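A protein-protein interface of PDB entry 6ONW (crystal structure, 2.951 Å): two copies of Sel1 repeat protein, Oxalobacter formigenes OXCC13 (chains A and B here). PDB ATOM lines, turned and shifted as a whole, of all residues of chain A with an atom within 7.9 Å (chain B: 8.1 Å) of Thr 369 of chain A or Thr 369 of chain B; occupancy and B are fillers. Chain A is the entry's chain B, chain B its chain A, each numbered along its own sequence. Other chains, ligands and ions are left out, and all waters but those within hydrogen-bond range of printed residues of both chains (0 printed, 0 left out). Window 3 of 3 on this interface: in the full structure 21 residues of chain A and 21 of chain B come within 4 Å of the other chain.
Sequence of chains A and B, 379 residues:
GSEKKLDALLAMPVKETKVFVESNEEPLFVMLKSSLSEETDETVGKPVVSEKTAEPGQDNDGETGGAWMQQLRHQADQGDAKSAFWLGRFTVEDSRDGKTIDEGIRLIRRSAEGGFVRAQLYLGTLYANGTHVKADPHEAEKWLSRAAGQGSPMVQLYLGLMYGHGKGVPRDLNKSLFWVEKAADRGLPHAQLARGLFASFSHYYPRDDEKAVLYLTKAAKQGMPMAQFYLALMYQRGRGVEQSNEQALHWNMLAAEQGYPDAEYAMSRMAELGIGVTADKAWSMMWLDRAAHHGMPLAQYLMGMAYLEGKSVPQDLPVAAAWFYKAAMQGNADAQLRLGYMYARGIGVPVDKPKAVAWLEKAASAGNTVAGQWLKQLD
Among the printed residues, merely in contact across the chains: Ala 333 of chain A with Gly 367 of chain B, Ala 366 of chain A with Ala 366 of chain B, Ala 366 of chain A with Gly 367 of chain B, Gly 367 of chain A with Asn 368 of chain B and Asn 368 of chain A with Thr 369 of chain B.
N of Asn 368 of chain A is in hydrogen-bond range of O of Gly 367 of chain B (3.3 Å). The backbone NH (N) of Asn 368 of chain B is in hydrogen-bond range of the backbone carbonyl oxygen (O) of Ala 366 of chain A (3.5 Å). The backbone NH (N) of Thr 369 of chain B is in hydrogen-bond range of the backbone carbonyl oxygen (O) of Gly 367 of chain A. OG1 of Thr 369 of chain B is in hydrogen-bond range of N of Thr 369 of chain A (3.2 Å). The backbone carbonyl oxygen of Gly 367 of chain A lies close to the backbone carbonyl oxygen of Gly 367 of chain B (3.4 Å).
Asp 334 of chain A touches none of the printed residues of chain B. Printed residues of chain B within 4 Å of Ala 366 of chain A: Ala 366, Gly 367 and Asn 368. Of chain B, only Gly 367 and Thr 369 come within 4 Å of Asn 368 of chain A. Of chain B, only Thr 369 (3.2 Å) comes within 4 Å of Thr 369 of chain A. Leu 360 of chain B touches none of the printed residues of chain A. Of the printed residues of chain A, Ala 366 of chain B touches Ala 366. Of the printed residues of chain A, Gly 367 of chain B touches Ala 333 (3.6 Å), Ala 366 (3.5 Å), Gly 367 (3.2 Å) and Asn 368 (3.3 Å). Of the printed residues of chain A, Asn 368 of chain B touches Ala 366 (3.5 Å) and Gly 367 (3.6 Å). Thr 369 of chain B touches just these residues of chain A: Gly 367 (2.8 Å), Asn 368 (3.4 Å) and Thr 369 (3.2 Å).
The backbone carbonyl oxygen (O) of Ala 363 of chain B sits close to the backbone NH (N) of Asn 368 of chain B. The side-chain amide oxygen of Asn 368 of chain B lies within hydrogen-bond range of the backbone NH of Ala 371 of chain B (3.0 Å). O of Ala 363 of chain A lies within hydrogen-bond range of N of Asn 368 of chain A, at 3.4 Å. The side-chain amide oxygen of Asn 368 of chain A lies within hydrogen-bond range of the backbone NH of Ala 371 of chain A (2.9 Å).
Hydrophobic or aromatic side chains of chain A that line the printed part of chain B: Ala 333 and Ala 366. Among the printed residues, no Asp or Glu carboxylate lies within 4 Å of a Lys or Arg side-chain nitrogen of the other chain.
Ala 366 of chain A touches its own counterpart, Ala 366 of chain B. Ala 366 of chain A touches Gly 367 of chain B, but with the chains exchanged Gly 367 of chain A does not touch Ala 366 of chain B (5.5 Å). Gly 367 of chain B touches its own counterpart, Gly 367 of chain A. Thr 369 of chain B touches its own counterpart, Thr 369 of chain A. 13 positions are printed for both chains. Of the 10 pairs that touch across the chains among the printed residues, 5 have their exchanged pair printed and touching as well.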
ATOM      1  N   PRO A  13     -22.962 -30.944   1.376  1.00  0.00           N
ATOM      2  CA  PRO A  13     -23.328 -29.570   1.018  1.00  0.00           C
ATOM      3  C   PRO A  13     -22.207 -28.867   0.270  1.00  0.00           C
ATOM      4  O   PRO A  13     -21.021 -29.083   0.526  1.00  0.00           O
ATOM      5  CB  PRO A  13     -23.588 -28.910   2.377  1.00  0.00           C
ATOM      6  CG  PRO A  13     -22.729 -29.677   3.326  1.00  0.00           C
ATOM      7  CD  PRO A  13     -22.725 -31.098   2.822  1.00  0.00           C
ATOM      8  N   ALA A 333     -10.546 -27.034   0.682  1.00  0.00           N
ATOM      9  CA  ALA A 333     -10.860 -28.082   1.646  1.00  0.00           C
ATOM     10  C   ALA A 333     -12.063 -28.921   1.240  1.00  0.00           C
ATOM     11  O   ALA A 333     -12.243 -30.018   1.779  1.00  0.00           O
ATOM     12  CB  ALA A 333     -11.093 -27.467   3.027  1.00  0.00           C
ATOM     13  N   ASP A 334     -12.892 -28.439   0.315  1.00  0.00           N
ATOM     14  CA  ASP A 334     -14.029 -29.220  -0.154  1.00  0.00           C
ATOM     15  C   ASP A 334     -13.660 -30.182  -1.276  1.00  0.00           C
ATOM     16  O   ASP A 334     -14.218 -31.283  -1.340  1.00  0.00           O
ATOM     17  CB  ASP A 334     -15.164 -28.293  -0.610  1.00  0.00           C
ATOM     18  CG  ASP A 334     -16.234 -28.107   0.454  1.00  0.00           C
ATOM     19  OD1 ASP A 334     -16.167 -27.110   1.206  1.00  0.00           O
ATOM     20  OD2 ASP A 334     -17.142 -28.963   0.540  1.00  0.00           O
ATOM     21  N   LEU A 337     -11.930 -33.035   0.669  1.00  0.00           N
ATOM     22  CA  LEU A 337     -12.916 -33.921   1.280  1.00  0.00           C
ATOM     23  C   LEU A 337     -13.576 -34.812   0.236  1.00  0.00           C
ATOM     24  O   LEU A 337     -13.729 -36.021   0.439  1.00  0.00           O
ATOM     25  CB  LEU A 337     -13.968 -33.099   2.024  1.00  0.00           C
ATOM     26  CG  LEU A 337     -15.356 -33.733   2.159  1.00  0.00           C
ATOM     27  CD1 LEU A 337     -15.348 -34.899   3.141  1.00  0.00           C
ATOM     28  CD2 LEU A 337     -16.378 -32.686   2.563  1.00  0.00           C
ATOM     29  N   ALA A 363      -7.902 -32.173   4.654  1.00  0.00           N
ATOM     30  CA  ALA A 363      -9.097 -31.341   4.735  1.00  0.00           C
ATOM     31  C   ALA A 363      -9.611 -31.236   6.164  1.00  0.00           C
ATOM     32  O   ALA A 363     -10.125 -30.186   6.564  1.00  0.00           O
ATOM     33  CB  ALA A 363     -10.191 -31.896   3.825  1.00  0.00           C
ATOM     34  N   ALA A 364      -9.499 -32.317   6.942  1.00  0.00           N
ATOM     35  CA  ALA A 364      -9.905 -32.260   8.342  1.00  0.00           C
ATOM     36  C   ALA A 364      -9.014 -31.318   9.139  1.00  0.00           C
ATOM     37  O   ALA A 364      -9.448 -30.765  10.155  1.00  0.00           O
ATOM     38  CB  ALA A 364      -9.888 -33.661   8.955  1.00  0.00           C
ATOM     39  N   ALA A 366      -8.015 -28.490   7.942  1.00  0.00           N
ATOM     40  CA  ALA A 366      -8.532 -27.167   7.621  1.00  0.00           C
ATOM     41  C   ALA A 366      -9.779 -26.809   8.420  1.00  0.00           C
ATOM     42  O   ALA A 366     -10.163 -25.636   8.441  1.00  0.00           O
ATOM     43  CB  ALA A 366      -8.836 -27.071   6.125  1.00  0.00           C
ATOM     44  N   GLY A 367     -10.411 -27.782   9.071  1.00  0.00           N
ATOM     45  CA  GLY A 367     -11.603 -27.540   9.853  1.00  0.00           C
ATOM     46  C   GLY A 367     -12.877 -28.141   9.301  1.00  0.00           C
ATOM     47  O   GLY A 367     -13.963 -27.775   9.764  1.00  0.00           O
ATOM     48  N   ASN A 368     -12.786 -29.046   8.330  1.00  0.00           N
ATOM     49  CA  ASN A 368     -13.968 -29.662   7.746  1.00  0.00           C
ATOM     50  C   ASN A 368     -14.491 -30.739   8.688  1.00  0.00           C
ATOM     51  O   ASN A 368     -13.809 -31.739   8.939  1.00  0.00           O
ATOM     52  CB  ASN A 368     -13.643 -30.247   6.375  1.00  0.00           C
ATOM     53  CG  ASN A 368     -14.884 -30.569   5.569  1.00  0.00           C
ATOM     54  OD1 ASN A 368     -15.494 -31.624   5.740  1.00  0.00           O
ATOM     55  ND2 ASN A 368     -15.264 -29.659   4.678  1.00  0.00           N
ATOM     56  N   THR A 369     -15.702 -30.532   9.212  1.00  0.00           N
ATOM     57  CA  THR A 369     -16.255 -31.451  10.202  1.00  0.00           C
ATOM     58  C   THR A 369     -16.499 -32.830   9.604  1.00  0.00           C
ATOM     59  O   THR A 369     -16.021 -33.842  10.132  1.00  0.00           O
ATOM     60  CB  THR A 369     -17.552 -30.880  10.778  1.00  0.00           C
ATOM     61  OG1 THR A 369     -17.269 -29.670  11.493  1.00  0.00           O
ATOM     62  CG2 THR A 369     -18.206 -31.883  11.717  1.00  0.00           C
ATOM     63  N   VAL A 370     -17.244 -32.891   8.497  1.00  0.00           N
ATOM     64  CA  VAL A 370     -17.602 -34.179   7.916  1.00  0.00           C
ATOM     65  C   VAL A 370     -16.387 -34.889   7.328  1.00  0.00           C
ATOM     66  O   VAL A 370     -16.429 -36.106   7.115  1.00  0.00           O
ATOM     67  CB  VAL A 370     -18.714 -33.993   6.863  1.00  0.00           C
ATOM     68  CG1 VAL A 370     -18.158 -33.382   5.595  1.00  0.00           C
ATOM     69  CG2 VAL A 370     -19.414 -35.317   6.574  1.00  0.00           C
ATOM     70  N   ALA A 371     -15.294 -34.166   7.072  1.00  0.00           N
ATOM     71  CA  ALA A 371     -14.076 -34.825   6.607  1.00  0.00           C
ATOM     72  C   ALA A 371     -13.464 -35.681   7.706  1.00  0.00           C
ATOM     73  O   ALA A 371     -12.939 -36.768   7.436  1.00  0.00           O
ATOM     74  CB  ALA A 371     -13.070 -33.789   6.108  1.00  0.00           C
ATOM     75  N   GLY A 372     -13.521 -35.207   8.954  1.00  0.00           N
ATOM     76  CA  GLY A 372     -13.038 -36.004  10.066  1.00  0.00           C
ATOM     77  C   GLY A 372     -13.961 -37.140  10.450  1.00  0.00           C
ATOM     78  O   GLY A 372     -13.511 -38.136  11.025  1.00  0.00           O
ATOM     79  N   GLN A 373     -15.256 -37.014  10.149  1.00  0.00           N
ATOM     80  CA  GLN A 373     -16.192 -38.092  10.452  1.00  0.00           C
ATOM     81  C   GLN A 373     -15.901 -39.322   9.604  1.00  0.00           C
ATOM     82  O   GLN A 373     -15.876 -40.449  10.114  1.00  0.00           O
ATOM     83  CB  GLN A 373     -17.630 -37.616  10.240  1.00  0.00           C
ATOM     84  CG  GLN A 373     -18.062 -36.509  11.186  1.00  0.00           C
ATOM     85  CD  GLN A 373     -19.502 -36.092  10.972  1.00  0.00           C
ATOM     86  OE1 GLN A 373     -20.132 -36.476   9.986  1.00  0.00           O
ATOM     87  NE2 GLN A 373     -20.035 -35.303  11.900  1.00  0.00           N
ATOM     88  N   TRP A 374     -15.673 -39.126   8.302  1.00  0.00           N
ATOM     89  CA  TRP A 374     -15.306 -40.248   7.444  1.00  0.00           C
ATOM     90  C   TRP A 374     -13.931 -40.794   7.798  1.00  0.00           C
ATOM     91  O   TRP A 374     -13.652 -41.973   7.552  1.00  0.00           O
ATOM     92  CB  TRP A 374     -15.349 -39.827   5.974  1.00  0.00           C
ATOM     93  CG  TRP A 374     -16.738 -39.701   5.434  1.00  0.00           C
ATOM     94  CD1 TRP A 374     -17.439 -38.548   5.232  1.00  0.00           C
ATOM     95  CD2 TRP A 374     -17.602 -40.772   5.035  1.00  0.00           C
ATOM     96  NE1 TRP A 374     -18.685 -38.834   4.727  1.00  0.00           N
ATOM     97  CE2 TRP A 374     -18.809 -40.192   4.598  1.00  0.00           C
ATOM     98  CE3 TRP A 374     -17.470 -42.163   5.004  1.00  0.00           C
ATOM     99  CZ2 TRP A 374     -19.878 -40.956   4.135  1.00  0.00           C
ATOM    100  CZ3 TRP A 374     -18.533 -42.919   4.544  1.00  0.00           C
ATOM    101  CH2 TRP A 374     -19.721 -42.314   4.115  1.00  0.00           C
ATOM    102  N   LEU A 375     -13.065 -39.960   8.373  1.00  0.00           N
ATOM    103  CA  LEU A 375     -11.760 -40.442   8.808  1.00  0.00           C
ATOM    104  C   LEU A 375     -11.896 -41.399   9.985  1.00  0.00           C
ATOM    105  O   LEU A 375     -11.153 -42.384  10.081  1.00  0.00           O
ATOM    106  CB  LEU A 375     -10.864 -39.258   9.169  1.00  0.00           C
ATOM    107  CG  LEU A 375      -9.356 -39.497   9.098  1.00  0.00           C
ATOM    108  CD1 LEU A 375      -8.954 -39.906   7.690  1.00  0.00           C
ATOM    109  CD2 LEU A 375      -8.596 -38.254   9.537  1.00  0.00           C
ATOM    110  N   LEU B 337     -11.135 -18.377  13.730  1.00  0.00           N
ATOM    111  CA  LEU B 337     -12.381 -18.905  14.273  1.00  0.00           C
ATOM    112  C   LEU B 337     -12.567 -18.488  15.727  1.00  0.00           C
ATOM    113  O   LEU B 337     -13.656 -18.060  16.126  1.00  0.00           O
ATOM    114  CB  LEU B 337     -12.398 -20.426  14.139  1.00  0.00           C
ATOM    115  CG  LEU B 337     -13.506 -21.176  14.874  1.00  0.00           C
ATOM    116  CD1 LEU B 337     -14.874 -20.794  14.334  1.00  0.00           C
ATOM    117  CD2 LEU B 337     -13.272 -22.668  14.755  1.00  0.00           C
ATOM    118  N   LEU B 360     -15.028 -14.656  10.627  1.00  0.00           N
ATOM    119  CA  LEU B 360     -15.693 -15.949  10.507  1.00  0.00           C
ATOM    120  C   LEU B 360     -15.734 -16.418   9.057  1.00  0.00           C
ATOM    121  O   LEU B 360     -15.298 -17.531   8.743  1.00  0.00           O
ATOM    122  CB  LEU B 360     -17.101 -15.878  11.096  1.00  0.00           C
ATOM    123  CG  LEU B 360     -17.184 -15.881  12.624  1.00  0.00           C
ATOM    124  CD1 LEU B 360     -18.630 -15.952  13.085  1.00  0.00           C
ATOM    125  CD2 LEU B 360     -16.377 -17.032  13.204  1.00  0.00           C
ATOM    126  N   ALA B 363     -12.465 -17.341   7.852  1.00  0.00           N
ATOM    127  CA  ALA B 363     -12.051 -18.666   8.294  1.00  0.00           C
ATOM    128  C   ALA B 363     -12.860 -19.775   7.645  1.00  0.00           C
ATOM    129  O   ALA B 363     -12.329 -20.870   7.421  1.00  0.00           O
ATOM    130  CB  ALA B 363     -12.168 -18.778   9.817  1.00  0.00           C
ATOM    131  N   ALA B 364     -14.136 -19.521   7.342  1.00  0.00           N
ATOM    132  CA  ALA B 364     -14.945 -20.520   6.656  1.00  0.00           C
ATOM    133  C   ALA B 364     -14.454 -20.755   5.235  1.00  0.00           C
ATOM    134  O   ALA B 364     -14.552 -21.876   4.723  1.00  0.00           O
ATOM    135  CB  ALA B 364     -16.413 -20.096   6.649  1.00  0.00           C
ATOM    136  N   SER B 365     -13.920 -19.717   4.587  1.00  0.00           N
ATOM    137  CA  SER B 365     -13.360 -19.887   3.250  1.00  0.00           C
ATOM    138  C   SER B 365     -12.153 -20.815   3.264  1.00  0.00           C
ATOM    139  O   SER B 365     -11.882 -21.495   2.268  1.00  0.00           O
ATOM    140  CB  SER B 365     -12.983 -18.527   2.663  1.00  0.00           C
ATOM    141  OG  SER B 365     -14.119 -17.686   2.566  1.00  0.00           O
ATOM    142  N   ALA B 366     -11.423 -20.860   4.377  1.00  0.00           N
ATOM    143  CA  ALA B 366     -10.297 -21.773   4.520  1.00  0.00           C
ATOM    144  C   ALA B 366     -10.728 -23.201   4.824  1.00  0.00           C
ATOM    145  O   ALA B 366      -9.864 -24.059   5.034  1.00  0.00           O
ATOM    146  CB  ALA B 366      -9.352 -21.275   5.616  1.00  0.00           C
ATOM    147  N   GLY B 367     -12.028 -23.475   4.861  1.00  0.00           N
ATOM    148  CA  GLY B 367     -12.526 -24.816   5.080  1.00  0.00           C
ATOM    149  C   GLY B 367     -13.027 -25.113   6.474  1.00  0.00           C
ATOM    150  O   GLY B 367     -13.377 -26.267   6.751  1.00  0.00           O
ATOM    151  N   ASN B 368     -13.076 -24.122   7.358  1.00  0.00           N
ATOM    152  CA  ASN B 368     -13.536 -24.335   8.725  1.00  0.00           C
ATOM    153  C   ASN B 368     -15.057 -24.435   8.720  1.00  0.00           C
ATOM    154  O   ASN B 368     -15.751 -23.450   8.448  1.00  0.00           O
ATOM    155  CB  ASN B 368     -13.054 -23.204   9.628  1.00  0.00           C
ATOM    156  CG  ASN B 368     -13.136 -23.560  11.093  1.00  0.00           C
ATOM    157  OD1 ASN B 368     -14.191 -23.439  11.712  1.00  0.00           O
ATOM    158  ND2 ASN B 368     -12.019 -24.006  11.658  1.00  0.00           N
ATOM    159  N   THR B 369     -15.577 -25.626   9.027  1.00  0.00           N
ATOM    160  CA  THR B 369     -17.015 -25.861   8.926  1.00  0.00           C
ATOM    161  C   THR B 369     -17.781 -25.117  10.014  1.00  0.00           C
ATOM    162  O   THR B 369     -18.766 -24.425   9.729  1.00  0.00           O
ATOM    163  CB  THR B 369     -17.306 -27.361   8.995  1.00  0.00           C
ATOM    164  OG1 THR B 369     -16.892 -27.987   7.775  1.00  0.00           O
ATOM    165  CG2 THR B 369     -18.790 -27.611   9.213  1.00  0.00           C
ATOM    166  N   VAL B 370     -17.346 -25.250  11.270  1.00  0.00           N
ATOM    167  CA  VAL B 370     -18.068 -24.642  12.381  1.00  0.00           C
ATOM    168  C   VAL B 370     -18.054 -23.120  12.295  1.00  0.00           C
ATOM    169  O   VAL B 370     -18.936 -22.459  12.856  1.00  0.00           O
ATOM    170  CB  VAL B 370     -17.488 -25.149  13.721  1.00  0.00           C
ATOM    171  CG1 VAL B 370     -16.052 -24.708  13.887  1.00  0.00           C
ATOM    172  CG2 VAL B 370     -18.333 -24.688  14.899  1.00  0.00           C
ATOM    173  N   ALA B 371     -17.084 -22.541  11.582  1.00  0.00           N
ATOM    174  CA  ALA B 371     -17.094 -21.097  11.366  1.00  0.00           C
ATOM    175  C   ALA B 371     -18.307 -20.675  10.545  1.00  0.00           C
ATOM    176  O   ALA B 371     -18.929 -19.644  10.826  1.00  0.00           O
ATOM    177  CB  ALA B 371     -15.800 -20.658  10.682  1.00  0.00           C
ATOM    178  N   GLY B 372     -18.659 -21.462   9.525  1.00  0.00           N
ATOM    179  CA  GLY B 372     -19.840 -21.171   8.732  1.00  0.00           C
ATOM    180  C   GLY B 372     -21.144 -21.467   9.440  1.00  0.00           C
ATOM    181  O   GLY B 372     -22.174 -20.880   9.091  1.00  0.00           O
ATOM    182  N   GLN B 373     -21.126 -22.368  10.425  1.00  0.00           N
ATOM    183  CA  GLN B 373     -22.329 -22.627  11.209  1.00  0.00           C
ATOM    184  C   GLN B 373     -22.659 -21.448  12.113  1.00  0.00           C
ATOM    185  O   GLN B 373     -23.826 -21.053  12.229  1.00  0.00           O
ATOM    186  CB  GLN B 373     -22.155 -23.904  12.029  1.00  0.00           C
ATOM    187  CG  GLN B 373     -21.892 -25.144  11.194  1.00  0.00           C
ATOM    188  CD  GLN B 373     -21.632 -26.369  12.045  1.00  0.00           C
ATOM    189  OE1 GLN B 373     -21.559 -26.282  13.270  1.00  0.00           O
ATOM    190  NE2 GLN B 373     -21.491 -27.520  11.399  1.00  0.00           N
ATOM    191  N   TRP B 374     -21.644 -20.875  12.767  1.00  0.00           N
ATOM    192  CA  TRP B 374     -21.856 -19.659  13.548  1.00  0.00           C
ATOM    193  C   TRP B 374     -22.196 -18.483  12.643  1.00  0.00           C
ATOM    194  O   TRP B 374     -23.026 -17.637  12.996  1.00  0.00           O
ATOM    195  CB  TRP B 374     -20.617 -19.348  14.387  1.00  0.00           C
ATOM    196  CG  TRP B 374     -20.403 -20.298  15.523  1.00  0.00           C
ATOM    197  CD1 TRP B 374     -21.313 -21.167  16.042  1.00  0.00           C
ATOM    198  CD2 TRP B 374     -19.200 -20.477  16.279  1.00  0.00           C
ATOM    199  NE1 TRP B 374     -20.755 -21.876  17.077  1.00  0.00           N
ATOM    200  CE2 TRP B 374     -19.457 -21.472  17.241  1.00  0.00           C
ATOM    201  CE3 TRP B 374     -17.931 -19.892  16.235  1.00  0.00           C
ATOM    202  CZ2 TRP B 374     -18.494 -21.896  18.153  1.00  0.00           C
ATOM    203  CZ3 TRP B 374     -16.975 -20.315  17.141  1.00  0.00           C
ATOM    204  CH2 TRP B 374     -17.261 -21.307  18.087  1.00  0.00           C
ATOM    205  N   LEU B 375     -21.558 -18.413  11.473  1.00  0.00           N
ATOM    206  CA  LEU B 375     -21.877 -17.364  10.513  1.00  0.00           C
ATOM    207  C   LEU B 375     -23.324 -17.460  10.047  1.00  0.00           C
ATOM    208  O   LEU B 375     -23.952 -16.438   9.753  1.00  0.00           O
ATOM    209  CB  LEU B 375     -20.924 -17.449   9.321  1.00  0.00           C
ATOM    210  CG  LEU B 375     -20.870 -16.253   8.375  1.00  0.00           C
ATOM    211  CD1 LEU B 375     -20.137 -15.091   9.027  1.00  0.00           C
ATOM    212  CD2 LEU B 375     -20.212 -16.646   7.064  1.00  0.00           C
ATOM    213  N   LYS B 376     -23.868 -18.679   9.982  1.00  0.00           N
ATOM    214  CA  LYS B 376     -25.262 -18.870   9.600  1.00  0.00           C
ATOM    215  C   LYS B 376     -26.226 -18.376  10.671  1.00  0.00           C
ATOM    216  O   LYS B 376     -27.403 -18.146  10.371  1.00  0.00           O
ATOM    217  CB  LYS B 376     -25.517 -20.351   9.308  1.00  0.00           C
ATOM    218  CG  LYS B 376     -26.725 -20.633   8.428  1.00  0.00           C
ATOM    219  CD  LYS B 376     -26.452 -20.258   6.981  1.00  0.00           C
ATOM    220  CE  LYS B 376     -27.614 -20.644   6.081  1.00  0.00           C
ATOM    221  NZ  LYS B 376     -27.346 -20.308   4.655  1.00  0.00           N
